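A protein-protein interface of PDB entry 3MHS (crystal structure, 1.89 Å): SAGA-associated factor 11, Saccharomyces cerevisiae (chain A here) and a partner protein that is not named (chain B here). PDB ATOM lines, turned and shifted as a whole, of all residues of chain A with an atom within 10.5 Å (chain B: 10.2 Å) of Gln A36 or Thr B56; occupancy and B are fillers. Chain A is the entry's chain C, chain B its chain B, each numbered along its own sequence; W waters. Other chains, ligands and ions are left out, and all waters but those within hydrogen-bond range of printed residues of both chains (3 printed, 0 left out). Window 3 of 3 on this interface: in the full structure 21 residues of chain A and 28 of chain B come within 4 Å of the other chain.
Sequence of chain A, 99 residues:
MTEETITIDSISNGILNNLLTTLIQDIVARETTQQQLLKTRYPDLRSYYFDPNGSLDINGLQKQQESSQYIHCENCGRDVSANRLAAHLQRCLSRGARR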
ATOM      1  N   ILE A  27      28.660   5.776  -0.215  1.00  0.00           N
ATOM      2  CA  ILE A  27      28.504   4.999   0.997  1.00  0.00           C
ATOM      3  C   ILE A  27      27.093   4.455   1.097  1.00  0.00           C
ATOM      4  O   ILE A  27      26.895   3.251   1.343  1.00  0.00           O
ATOM      5  CB  ILE A  27      28.810   5.843   2.259  1.00  0.00           C
ATOM      6  CG1 ILE A  27      30.302   6.229   2.301  1.00  0.00           C
ATOM      7  CG2 ILE A  27      28.413   5.064   3.516  1.00  0.00           C
ATOM      8  CD1 ILE A  27      30.570   7.337   3.273  1.00  0.00           C
ATOM      9  N   VAL A  28      26.104   5.311   0.855  1.00  0.00           N
ATOM     10  CA  VAL A  28      24.717   4.862   1.013  1.00  0.00           C
ATOM     11  C   VAL A  28      24.361   3.778  -0.037  1.00  0.00           C
ATOM     12  O   VAL A  28      23.696   2.797   0.275  1.00  0.00           O
ATOM     13  CB  VAL A  28      23.713   6.038   0.964  1.00  0.00           C
ATOM     14  CG1 VAL A  28      22.269   5.528   0.916  1.00  0.00           C
ATOM     15  CG2 VAL A  28      23.914   6.975   2.156  1.00  0.00           C
ATOM     16  N   ALA A  29      24.797   3.965  -1.276  1.00  0.00           N
ATOM     17  CA  ALA A  29      24.548   2.988  -2.338  1.00  0.00           C
ATOM     18  C   ALA A  29      25.150   1.643  -2.011  1.00  0.00           C
ATOM     19  O   ALA A  29      24.562   0.622  -2.299  1.00  0.00           O
ATOM     20  CB  ALA A  29      25.064   3.496  -3.689  1.00  0.00           C
ATOM     21  N   ARG A  30      26.334   1.633  -1.399  1.00  0.00           N
ATOM     22  CA  ARG A  30      26.957   0.384  -1.018  1.00  0.00           C
ATOM     23  C   ARG A  30      26.152  -0.317   0.097  1.00  0.00           C
ATOM     24  O   ARG A  30      25.957  -1.529   0.054  1.00  0.00           O
ATOM     25  CB  ARG A  30      28.415   0.600  -0.626  1.00  0.00           C
ATOM     26  CG  ARG A  30      29.348   1.006  -1.797  1.00  0.00           C
ATOM     27  CD  ARG A  30      30.709   1.466  -1.294  1.00  0.00           C
ATOM     28  NE  ARG A  30      31.578   2.057  -2.321  1.00  0.00           N
ATOM     29  CZ  ARG A  30      32.735   1.546  -2.739  1.00  0.00           C
ATOM     30  NH1 ARG A  30      33.184   0.415  -2.255  1.00  0.00           N
ATOM     31  NH2 ARG A  30      33.451   2.175  -3.665  1.00  0.00           N
ATOM     32  N   GLU A  31      25.658   0.451   1.057  1.00  0.00           N
ATOM     33  CA  GLU A  31      24.860  -0.082   2.161  1.00  0.00           C
ATOM     34  C   GLU A  31      23.517  -0.653   1.668  1.00  0.00           C
ATOM     35  O   GLU A  31      23.125  -1.757   2.051  1.00  0.00           O
ATOM     36  CB  GLU A  31      24.587   1.046   3.175  1.00  0.00           C
ATOM     37  CG  GLU A  31      25.806   1.434   3.999  1.00  0.00           C
ATOM     38  CD  GLU A  31      26.371   0.231   4.719  1.00  0.00           C
ATOM     39  OE1 GLU A  31      25.574  -0.556   5.298  1.00  0.00           O
ATOM     40  OE2 GLU A  31      27.576   0.037   4.655  1.00  0.00           O
ATOM     41  N   THR A  32      22.815   0.099   0.834  1.00  0.00           N
ATOM     42  CA  THR A  32      21.465  -0.309   0.420  1.00  0.00           C
ATOM     43  C   THR A  32      21.527  -1.535  -0.500  1.00  0.00           C
ATOM     44  O   THR A  32      20.731  -2.458  -0.326  1.00  0.00           O
ATOM     45  CB  THR A  32      20.669   0.815  -0.235  1.00  0.00           C
ATOM     46  OG1 THR A  32      21.348   1.276  -1.407  1.00  0.00           O
ATOM     47  CG2 THR A  32      20.427   1.966   0.730  1.00  0.00           C
ATOM     48  N   THR A  33      22.512  -1.586  -1.408  1.00  0.00           N
ATOM     49  CA  THR A  33      22.686  -2.743  -2.294  1.00  0.00           C
ATOM     50  C   THR A  33      23.038  -3.985  -1.497  1.00  0.00           C
ATOM     51  O   THR A  33      22.496  -5.060  -1.737  1.00  0.00           O
ATOM     52  CB  THR A  33      23.758  -2.507  -3.423  1.00  0.00           C
ATOM     53  OG1 THR A  33      24.982  -2.011  -2.873  1.00  0.00           O
ATOM     54  CG2 THR A  33      23.243  -1.511  -4.449  1.00  0.00           C
ATOM     55  N   GLN A  34      23.915  -3.843  -0.520  1.00  0.00           N
ATOM     56  CA  GLN A  34      24.311  -4.999   0.302  1.00  0.00           C
ATOM     57  C   GLN A  34      23.119  -5.562   1.075  1.00  0.00           C
ATOM     58  O   GLN A  34      22.954  -6.776   1.179  1.00  0.00           O
ATOM     59  CB  GLN A  34      25.400  -4.591   1.321  1.00  0.00           C
ATOM     60  CG  GLN A  34      26.720  -4.362   0.718  1.00  0.00           C
ATOM     61  CD  GLN A  34      27.792  -4.082   1.790  1.00  0.00           C
ATOM     62  OE1 GLN A  34      28.715  -3.285   1.570  1.00  0.00           O
ATOM     63  NE2 GLN A  34      27.644  -4.716   2.959  1.00  0.00           N
ATOM     64  N   GLN A  35      22.324  -4.666   1.640  1.00  0.00           N
ATOM     65  CA  GLN A  35      21.182  -5.063   2.476  1.00  0.00           C
ATOM     66  C   GLN A  35      20.066  -5.647   1.617  1.00  0.00           C
ATOM     67  O   GLN A  35      19.428  -6.655   1.993  1.00  0.00           O
ATOM     68  CB  GLN A  35      20.695  -3.889   3.301  1.00  0.00           C
ATOM     69  CG  GLN A  35      19.571  -4.242   4.308  1.00  0.00           C
ATOM     70  CD  GLN A  35      20.008  -5.239   5.371  1.00  0.00           C
ATOM     71  OE1 GLN A  35      21.131  -5.730   5.357  1.00  0.00           O
ATOM     72  NE2 GLN A  35      19.110  -5.548   6.296  1.00  0.00           N
ATOM     73  N   GLN A  36      19.860  -5.057   0.445  1.00  0.00           N
ATOM     74  CA  GLN A  36      18.931  -5.628  -0.522  1.00  0.00           C
ATOM     75  C   GLN A  36      19.323  -7.066  -0.862  1.00  0.00           C
ATOM     76  O   GLN A  36      18.467  -7.928  -0.898  1.00  0.00           O
ATOM     77  CB  GLN A  36      18.849  -4.804  -1.814  1.00  0.00           C
ATOM     78  CG  GLN A  36      17.717  -5.297  -2.708  1.00  0.00           C
ATOM     79  CD  GLN A  36      17.705  -4.687  -4.093  1.00  0.00           C
ATOM     80  OE1 GLN A  36      18.732  -4.631  -4.774  1.00  0.00           O
ATOM     81  NE2 GLN A  36      16.502  -4.284  -4.550  1.00  0.00           N
ATOM     82  N   LEU A  37      20.606  -7.310  -1.121  1.00  0.00           N
ATOM     83  CA  LEU A  37      21.090  -8.665  -1.422  1.00  0.00           C
ATOM     84  C   LEU A  37      20.858  -9.627  -0.232  1.00  0.00           C
ATOM     85  O   LEU A  37      20.301 -10.713  -0.408  1.00  0.00           O
ATOM     86  CB  LEU A  37      22.573  -8.651  -1.798  1.00  0.00           C
ATOM     87  CG  LEU A  37      23.218 -10.017  -2.080  1.00  0.00           C
ATOM     88  CD1 LEU A  37      22.535 -10.713  -3.259  1.00  0.00           C
ATOM     89  CD2 LEU A  37      24.728  -9.915  -2.300  1.00  0.00           C
ATOM     90  N   LEU A  38      21.240  -9.206   0.975  1.00  0.00           N
ATOM     91  CA  LEU A  38      21.158 -10.080   2.154  1.00  0.00           C
ATOM     92  C   LEU A  38      19.687 -10.449   2.405  1.00  0.00           C
ATOM     93  O   LEU A  38      19.369 -11.611   2.619  1.00  0.00           O
ATOM     94  CB  LEU A  38      21.708  -9.373   3.395  1.00  0.00           C
ATOM     95  CG  LEU A  38      23.122  -9.569   3.883  1.00  0.00           C
ATOM     96  CD1 LEU A  38      23.140  -8.964   5.309  1.00  0.00           C
ATOM     97  CD2 LEU A  38      23.537 -11.018   3.898  1.00  0.00           C
ATOM     98  N   LYS A  39      18.805  -9.464   2.307  1.00  0.00           N
ATOM     99  CA  LYS A  39      17.379  -9.678   2.504  1.00  0.00           C
ATOM    100  C   LYS A  39      16.744 -10.566   1.446  1.00  0.00           C
ATOM    101  O   LYS A  39      15.822 -11.307   1.763  1.00  0.00           O
ATOM    102  CB  LYS A  39      16.611  -8.355   2.599  1.00  0.00           C
ATOM    103  CG  LYS A  39      16.854  -7.605   3.920  1.00  0.00           C
ATOM    104  CD  LYS A  39      16.230  -6.195   3.945  1.00  0.00           C
ATOM    105  CE  LYS A  39      14.704  -6.202   4.120  1.00  0.00           C
ATOM    106  NZ  LYS A  39      14.163  -4.822   3.891  1.00  0.00           N
ATOM    107  N   THR A  40      17.217 -10.484   0.201  1.00  0.00           N
ATOM    108  CA  THR A  40      16.710 -11.325  -0.887  1.00  0.00           C
ATOM    109  C   THR A  40      17.279 -12.723  -0.737  1.00  0.00           C
ATOM    110  O   THR A  40      16.589 -13.733  -0.887  1.00  0.00           O
ATOM    111  CB  THR A  40      17.105 -10.753  -2.289  1.00  0.00           C
ATOM    112  OG1 THR A  40      16.677  -9.387  -2.389  1.00  0.00           O
ATOM    113  CG2 THR A  40      16.473 -11.576  -3.425  1.00  0.00           C
ATOM    114  N   ARG A  41      18.558 -12.777  -0.431  1.00  0.00           N
ATOM    115  CA  ARG A  41      19.248 -14.047  -0.261  1.00  0.00           C
ATOM    116  C   ARG A  41      18.730 -14.824   0.945  1.00  0.00           C
ATOM    117  O   ARG A  41      18.620 -16.048   0.891  1.00  0.00           O
ATOM    118  CB  ARG A  41      20.751 -13.787  -0.102  1.00  0.00           C
ATOM    119  CG  ARG A  41      21.611 -15.002  -0.278  1.00  0.00           C
ATOM    120  CD  ARG A  41      23.065 -14.616  -0.328  1.00  0.00           C
ATOM    121  NE  ARG A  41      23.553 -14.430  -1.693  1.00  0.00           N
ATOM    122  CZ  ARG A  41      24.839 -14.296  -2.005  1.00  0.00           C
ATOM    123  NH1 ARG A  41      25.767 -14.316  -1.056  1.00  0.00           N
ATOM    124  NH2 ARG A  41      25.198 -14.159  -3.269  1.00  0.00           N
ATOM    125  N   TYR A  42      18.425 -14.107   2.026  1.00  0.00           N
ATOM    126  CA  TYR A  42      18.108 -14.727   3.311  1.00  0.00           C
ATOM    127  C   TYR A  42      16.797 -14.153   3.853  1.00  0.00           C
ATOM    128  O   TYR A  42      16.810 -13.299   4.754  1.00  0.00           O
ATOM    129  CB  TYR A  42      19.248 -14.478   4.316  1.00  0.00           C
ATOM    130  CG  TYR A  42      20.592 -14.983   3.862  1.00  0.00           C
ATOM    131  CD1 TYR A  42      20.769 -16.318   3.501  1.00  0.00           C
ATOM    132  CD2 TYR A  42      21.690 -14.140   3.799  1.00  0.00           C
ATOM    133  CE1 TYR A  42      22.016 -16.800   3.117  1.00  0.00           C
ATOM    134  CE2 TYR A  42      22.948 -14.617   3.390  1.00  0.00           C
ATOM    135  CZ  TYR A  42      23.098 -15.931   3.044  1.00  0.00           C
ATOM    136  OH  TYR A  42      24.326 -16.414   2.641  1.00  0.00           O
ATOM    137  N   PRO A  43      15.657 -14.601   3.301  1.00  0.00           N
ATOM    138  CA  PRO A  43      14.353 -14.044   3.714  1.00  0.00           C
ATOM    139  C   PRO A  43      14.137 -14.069   5.232  1.00  0.00           C
ATOM    140  O   PRO A  43      13.542 -13.138   5.782  1.00  0.00           O
ATOM    141  CB  PRO A  43      13.337 -14.948   3.016  1.00  0.00           C
ATOM    142  CG  PRO A  43      14.087 -15.617   1.908  1.00  0.00           C
ATOM    143  CD  PRO A  43      15.514 -15.701   2.329  1.00  0.00           C
ATOM    144  N   LEU A  45      16.489 -13.919   7.524  1.00  0.00           N
ATOM    145  CA  LEU A  45      17.678 -13.337   8.143  1.00  0.00           C
ATOM    146  C   LEU A  45      17.372 -12.817   9.524  1.00  0.00           C
ATOM    147  O   LEU A  45      16.434 -12.054   9.705  1.00  0.00           O
ATOM    148  CB  LEU A  45      18.197 -12.164   7.303  1.00  0.00           C
ATOM    149  CG  LEU A  45      19.482 -11.511   7.836  1.00  0.00           C
ATOM    150  CD1 LEU A  45      20.603 -12.535   7.875  1.00  0.00           C
ATOM    151  CD2 LEU A  45      19.875 -10.314   6.998  1.00  0.00           C
ATOM    152  N   THR B  46      22.940   4.751   8.063  1.00  0.00           N
ATOM    153  CA  THR B  46      22.237   4.183   6.909  1.00  0.00           C
ATOM    154  C   THR B  46      21.536   2.869   7.295  1.00  0.00           C
ATOM    155  O   THR B  46      20.372   2.665   6.942  1.00  0.00           O
ATOM    156  CB  THR B  46      23.176   3.986   5.655  1.00  0.00           C
ATOM    157  OG1 THR B  46      23.816   5.230   5.317  1.00  0.00           O
ATOM    158  CG2 THR B  46      22.383   3.511   4.437  1.00  0.00           C
ATOM    159  N   LYS B  47      22.204   2.013   8.066  1.00  0.00           N
ATOM    160  CA  LYS B  47      21.599   0.759   8.492  1.00  0.00           C
ATOM    161  C   LYS B  47      20.372   1.050   9.374  1.00  0.00           C
ATOM    162  O   LYS B  47      19.347   0.388   9.258  1.00  0.00           O
ATOM    163  CB  LYS B  47      22.586  -0.085   9.287  1.00  0.00           C
ATOM    164  CG  LYS B  47      23.860  -0.454   8.560  1.00  0.00           C
ATOM    165  CD  LYS B  47      23.867  -1.889   8.084  1.00  0.00           C
ATOM    166  CE  LYS B  47      25.216  -2.542   8.367  1.00  0.00           C
ATOM    167  NZ  LYS B  47      26.351  -1.798   7.751  1.00  0.00           N
ATOM    168  N   SER B  48      20.507   2.044  10.251  1.00  0.00           N
ATOM    169  CA  SER B  48      19.444   2.460  11.155  1.00  0.00           C
ATOM    170  C   SER B  48      18.215   2.971  10.393  1.00  0.00           C
ATOM    171  O   SER B  48      17.083   2.606  10.713  1.00  0.00           O
ATOM    172  CB  SER B  48      19.971   3.556  12.093  1.00  0.00           C
ATOM    173  OG  SER B  48      18.995   3.907  13.056  1.00  0.00           O
ATOM    174  N   GLU B  49      18.446   3.799   9.377  1.00  0.00           N
ATOM    175  CA  GLU B  49      17.359   4.336   8.573  1.00  0.00           C
ATOM    176  C   GLU B  49      16.675   3.240   7.769  1.00  0.00           C
ATOM    177  O   GLU B  49      15.448   3.226   7.630  1.00  0.00           O
ATOM    178  CB  GLU B  49      17.877   5.440   7.656  1.00  0.00           C
ATOM    179  CG  GLU B  49      18.279   6.718   8.413  1.00  0.00           C
ATOM    180  CD  GLU B  49      17.109   7.382   9.126  1.00  0.00           C
ATOM    181  OE1 GLU B  49      16.038   7.535   8.515  1.00  0.00           O
ATOM    182  OE2 GLU B  49      17.255   7.724  10.312  1.00  0.00           O
ATOM    183  N   MET B  50      17.458   2.309   7.248  1.00  0.00           N
ATOM    184  CA  MET B  50      16.873   1.147   6.573  1.00  0.00           C
ATOM    185  C   MET B  50      15.967   0.354   7.536  1.00  0.00           C
ATOM    186  O   MET B  50      14.919  -0.157   7.131  1.00  0.00           O
ATOM    187  CB  MET B  50      17.966   0.250   5.979  1.00  0.00           C
ATOM    188  CG  MET B  50      18.580   0.806   4.692  1.00  0.00           C
ATOM    189  SD  MET B  50      19.694  -0.333   3.811  1.00  0.00           S
ATOM    190  CE  MET B  50      21.098  -0.330   4.918  1.00  0.00           C
ATOM    191  N   ASN B  51      16.368   0.244   8.803  1.00  0.00           N
ATOM    192  CA  ASN B  51      15.570  -0.510   9.776  1.00  0.00           C
ATOM    193  C   ASN B  51      14.313   0.232  10.220  1.00  0.00           C
ATOM    194  O   ASN B  51      13.265  -0.384  10.409  1.00  0.00           O
ATOM    195  CB  ASN B  51      16.405  -0.908  10.999  1.00  0.00           C
ATOM    196  CG  ASN B  51      17.397  -2.028  10.691  1.00  0.00           C
ATOM    197  OD1 ASN B  51      17.093  -2.957   9.930  1.00  0.00           O
ATOM    198  ND2 ASN B  51      18.583  -1.950  11.285  1.00  0.00           N
ATOM    199  N   ILE B  52      14.430   1.554  10.342  1.00  0.00           N
ATOM    200  CA  ILE B  52      13.335   2.413  10.768  1.00  0.00           C
ATOM    201  C   ILE B  52      12.286   2.509   9.676  1.00  0.00           C
ATOM    202  O   ILE B  52      11.093   2.512   9.953  1.00  0.00           O
ATOM    203  CB  ILE B  52      13.828   3.834  11.075  1.00  0.00           C
ATOM    204  CG1 ILE B  52      14.622   3.843  12.376  1.00  0.00           C
ATOM    205  CG2 ILE B  52      12.659   4.800  11.203  1.00  0.00           C
ATOM    206  CD1 ILE B  52      15.550   5.041  12.494  1.00  0.00           C
ATOM    207  N   ASN B  53      12.750   2.595   8.433  1.00  0.00           N
ATOM    208  CA  ASN B  53      11.856   2.755   7.300  1.00  0.00           C
ATOM    209  C   ASN B  53      11.517   1.441   6.597  1.00  0.00           C
ATOM    210  O   ASN B  53      10.664   1.421   5.697  1.00  0.00           O
ATOM    211  CB  ASN B  53      12.437   3.777   6.328  1.00  0.00           C
ATOM    212  CG  ASN B  53      12.410   5.185   6.900  1.00  0.00           C
ATOM    213  OD1 ASN B  53      11.348   5.778   7.028  1.00  0.00           O
ATOM    214  ND2 ASN B  53      13.570   5.708   7.277  1.00  0.00           N
ATOM    215  N   GLU B  54      12.129   0.343   7.056  1.00  0.00           N
ATOM    216  CA  GLU B  54      11.854  -1.000   6.517  1.00  0.00           C
ATOM    217  C   GLU B  54      11.973  -0.992   4.992  1.00  0.00           C
ATOM    218  O   GLU B  54      11.068  -1.416   4.270  1.00  0.00           O
ATOM    219  CB  GLU B  54      10.449  -1.479   6.927  1.00  0.00           C
ATOM    220  CG  GLU B  54      10.232  -1.589   8.435  1.00  0.00           C
ATOM    221  CD  GLU B  54       8.865  -2.147   8.804  1.00  0.00           C
ATOM    222  OE1 GLU B  54       8.412  -1.897   9.942  1.00  0.00           O
ATOM    223  OE2 GLU B  54       8.235  -2.828   7.966  1.00  0.00           O
ATOM    224  N   SER B  55      13.094  -0.483   4.511  1.00  0.00           N
ATOM    225  CA  SER B  55      13.257  -0.195   3.104  1.00  0.00           C
ATOM    226  C   SER B  55      14.738  -0.205   2.786  1.00  0.00           C
ATOM    227  O   SER B  55      15.554   0.161   3.630  1.00  0.00           O
ATOM    228  CB  SER B  55      12.661   1.183   2.793  1.00  0.00           C
ATOM    229  OG  SER B  55      12.882   1.571   1.445  1.00  0.00           O
ATOM    230  N   THR B  56      15.073  -0.678   1.592  1.00  0.00           N
ATOM    231  CA  THR B  56      16.419  -0.539   1.054  1.00  0.00           C
ATOM    232  C   THR B  56      16.386   0.353  -0.194  1.00  0.00           C
ATOM    233  O   THR B  56      17.357   0.385  -0.949  1.00  0.00           O
ATOM    234  CB  THR B  56      17.055  -1.915   0.688  1.00  0.00           C
ATOM    235  OG1 THR B  56      16.252  -2.584  -0.296  1.00  0.00           O
ATOM    236  CG2 THR B  56      17.208  -2.812   1.920  1.00  0.00           C
ATOM    237  N   ASN B  57      15.278   1.077  -0.411  1.00  0.00           N
ATOM    238  CA  ASN B  57      15.169   1.971  -1.567  1.00  0.00           C
ATOM    239  C   ASN B  57      16.131   3.131  -1.413  1.00  0.00           C
ATOM    240  O   ASN B  57      16.085   3.879  -0.428  1.00  0.00           O
ATOM    241  CB  ASN B  57      13.737   2.482  -1.781  1.00  0.00           C
ATOM    242  CG  ASN B  57      13.597   3.327  -3.057  1.00  0.00           C
ATOM    243  OD1 ASN B  57      13.122   2.842  -4.092  1.00  0.00           O
ATOM    244  ND2 ASN B  57      14.014   4.585  -2.986  1.00  0.00           N
ATOM    245  N   PHE B  58      17.033   3.250  -2.387  1.00  0.00           N
ATOM    246  CA  PHE B  58      18.167   4.155  -2.269  1.00  0.00           C
ATOM    247  C   PHE B  58      17.704   5.594  -2.190  1.00  0.00           C
ATOM    248  O   PHE B  58      18.209   6.361  -1.398  1.00  0.00           O
ATOM    249  CB  PHE B  58      19.136   3.986  -3.444  1.00  0.00           C
ATOM    250  CG  PHE B  58      20.198   5.041  -3.490  1.00  0.00           C
ATOM    251  CD1 PHE B  58      21.310   4.949  -2.689  1.00  0.00           C
ATOM    252  CD2 PHE B  58      20.041   6.156  -4.284  1.00  0.00           C
ATOM    253  CE1 PHE B  58      22.254   5.956  -2.685  1.00  0.00           C
ATOM    254  CE2 PHE B  58      20.975   7.147  -4.295  1.00  0.00           C
ATOM    255  CZ  PHE B  58      22.078   7.056  -3.487  1.00  0.00           C
ATOM    256  N   THR B  59      16.731   5.956  -3.013  1.00  0.00           N
ATOM    257  CA  THR B  59      16.271   7.342  -3.071  1.00  0.00           C
ATOM    258  C   THR B  59      15.650   7.777  -1.761  1.00  0.00           C
ATOM    259  O   THR B  59      16.006   8.831  -1.240  1.00  0.00           O
ATOM    260  CB  THR B  59      15.304   7.573  -4.248  1.00  0.00           C
ATOM    261  OG1 THR B  59      16.019   7.326  -5.462  1.00  0.00           O
ATOM    262  CG2 THR B  59      14.780   9.000  -4.246  1.00  0.00           C
ATOM    263  N   GLN B  60      14.766   6.958  -1.201  1.00  0.00           N
ATOM    264  CA  GLN B  60      14.135   7.313   0.070  1.00  0.00           C
ATOM    265  C   GLN B  60      15.102   7.231   1.259  1.00  0.00           C
ATOM    266  O   GLN B  60      15.025   8.057   2.168  1.00  0.00           O
ATOM    267  CB  GLN B  60      12.845   6.520   0.325  1.00  0.00           C
ATOM    268  CG  GLN B  60      13.006   5.098   0.794  1.00  0.00           C
ATOM    269  CD  GLN B  60      11.704   4.511   1.333  1.00  0.00           C
ATOM    270  OE1 GLN B  60      11.262   4.852   2.432  1.00  0.00           O
ATOM    271  NE2 GLN B  60      11.090   3.615   0.561  1.00  0.00           N
ATOM    272  N   ILE B  61      16.027   6.273   1.254  1.00  0.00           N
ATOM    273  CA  ILE B  61      16.995   6.193   2.339  1.00  0.00           C
ATOM    274  C   ILE B  61      17.973   7.377   2.287  1.00  0.00           C
ATOM    275  O   ILE B  61      18.300   7.966   3.318  1.00  0.00           O
ATOM    276  CB  ILE B  61      17.782   4.856   2.339  1.00  0.00           C
ATOM    277  CG1 ILE B  61      16.851   3.686   2.668  1.00  0.00           C
ATOM    278  CG2 ILE B  61      18.956   4.917   3.346  1.00  0.00           C
ATOM    279  CD1 ILE B  61      15.992   3.905   3.930  1.00  0.00           C
ATOM    280  N   LEU B  62      18.438   7.728   1.095  1.00  0.00           N
ATOM    281  CA  LEU B  62      19.349   8.853   0.943  1.00  0.00           C
ATOM    282  C   LEU B  62      18.733  10.154   1.453  1.00  0.00           C
ATOM    283  O   LEU B  62      19.427  11.009   2.011  1.00  0.00           O
ATOM    284  CB  LEU B  62      19.735   9.023  -0.527  1.00  0.00           C
ATOM    285  CG  LEU B  62      20.774  10.115  -0.836  1.00  0.00           C
ATOM    286  CD1 LEU B  62      22.207   9.750  -0.298  1.00  0.00           C
ATOM    287  CD2 LEU B  62      20.806  10.376  -2.325  1.00  0.00           C
ATOM    288  N   SER B  63      17.431  10.314   1.241  1.00  0.00           N
ATOM    289  CA  SER B  63      16.749  11.557   1.590  1.00  0.00           C
ATOM    290  C   SER B  63      16.837  11.851   3.092  1.00  0.00           C
ATOM    291  O   SER B  63      16.781  13.018   3.507  1.00  0.00           O
ATOM    292  CB  SER B  63      15.282  11.491   1.158  1.00  0.00           C
ATOM    293  OG  SER B  63      14.550  10.630   2.011  1.00  0.00           O
ATOM    294  N   VAL B  65      19.303  10.088   5.169  1.00  0.00           N
ATOM    295  CA  VAL B  65      20.718   9.952   5.560  1.00  0.00           C
ATOM    296  C   VAL B  65      21.563  11.170   5.192  1.00  0.00           C
ATOM    297  O   VAL B  65      22.315  11.685   6.024  1.00  0.00           O
ATOM    298  CB  VAL B  65      21.367   8.712   4.943  1.00  0.00           C
ATOM    299  CG1 VAL B  65      22.868   8.649   5.319  1.00  0.00           C
ATOM    300  CG2 VAL B  65      20.636   7.470   5.403  1.00  0.00           C
HETATM  301  O   HOH W   1      17.402  -1.607  -2.624  1.00  0.00           O
HETATM  302  O   HOH W   2      15.639  -3.077   5.441  1.00  0.00           O
HETATM  303  O   HOH W   3      28.770  -1.855   5.909  1.00  0.00           O
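CG2 of Val A28 touches OG1 of Thr B46, at 3.6 Å. CG1 of Val A28 touches CE1 of Phe B58, 3.6 Å away. Val B65 touches Val A28 (CG1 to CG2, 3.7 Å). Phe B58 touches Ala A29 (CE1 to N, 3.5 Å). Glu A31 touches Thr B46. Met B50 touches Glu A31 (CE to O, 3.8 Å). Thr A32 touches Phe B58. Gln A35 touches Met B50 (CB to SD, 3.7 Å). CG of Gln A35 touches CG2 of Thr B56 (3.7 Å). Thr B56 touches Gln A36.
Of the 18 printed residues of chain A, 6 touch a printed residue of chain B. Hydrophobic or aromatic side chains of chain A within 4 Å of the printed part of chain B: Val A28 and Ala A29. Of the 19 printed residues of chain B, 6 touch a printed residue of chain A. Printed residues of chain B that touch a printed residue of chain A: Thr B46, Lys B47, Met B50, Thr B56, Phe B58 and Val B65. Among the printed residues, Asp or Glu carboxylates within 4 Å of a Lys or Arg side-chain nitrogen of the other chain: Glu A31 with Lys B47 (2.9 Å).
Gln A36 touches just one residue of chain B: Thr B56 (3.7 Å). Thr B56 touches just these residues of chain A: Thr A32 (3.4 Å), Gln A35 (3.7 Å) and Gln A36 (3.7 Å). Gln A35 touches just these residues of chain B: Met B50 (3.7 Å) and Thr B56 (3.7 Å). Thr A40 touches none of the printed residues of chain B. No residue of chain A comes within 4 Å of Ser B55. No residue of chain A comes within 4 Å of Asn B57. Of the printed residues of chain B, Val A28 touches Thr B46 (3.6 Å), Phe B58 (3.6 Å) and Val B65 (3.7 Å). Of the printed residues of chain A, Lys B47 touches Glu A31 (2.9 Å). Of the printed residues of chain A, Val B65 touches Val A28. Printed residues of chain B within 4 Å of Ala A29: Phe B58. Tyr A42 touches none of the printed residues of chain B.
The backbone carbonyl oxygen (O) of Gln A36 lies within hydrogen-bond range of the side-chain hydroxyl (OG1) of Thr A40, 2.7 Å away. O of Ala A29 sits at hydrogen-bond distance from OG1 of Thr A33 (2.7 Å). The backbone carbonyl oxygen of Val A28 is in hydrogen-bond range of the side-chain hydroxyl of Thr A32 (3.3 Å). O of Ala A29 lies within hydrogen-bond range of OG1 of Thr A32 (3.4 Å). The backbone carbonyl oxygen of Met B50 is in hydrogen-bond range of the backbone NH of Ser B55 (3.2 Å). The backbone carbonyl oxygen (O) of Lys B47 lies within hydrogen-bond range of the side-chain amide nitrogen (ND2) of Asn B51, at 3.2 Å.
Water W3 lies within hydrogen-bond range of the side-chain carboxylate of Glu A31 (2.6 Å) and the side-chain amino group of Lys B47 (3.0 Å). Water W1 bridges the backbone carbonyl oxygen (O) of Thr B56 (2.6 Å) and the side-chain amide nitrogen (NE2) of Gln A36 (3.4 Å). Water W2 lies within hydrogen-bond range of the side-chain amino group (NZ) of Lys A39 (2.8 Å) and the backbone carbonyl oxygen (O) of Met B50 (3.4 Å).
The side-chain amino group of Lys B47 is in salt-bridge range of the side-chain carboxylate of Glu A31, at 2.9 Å.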
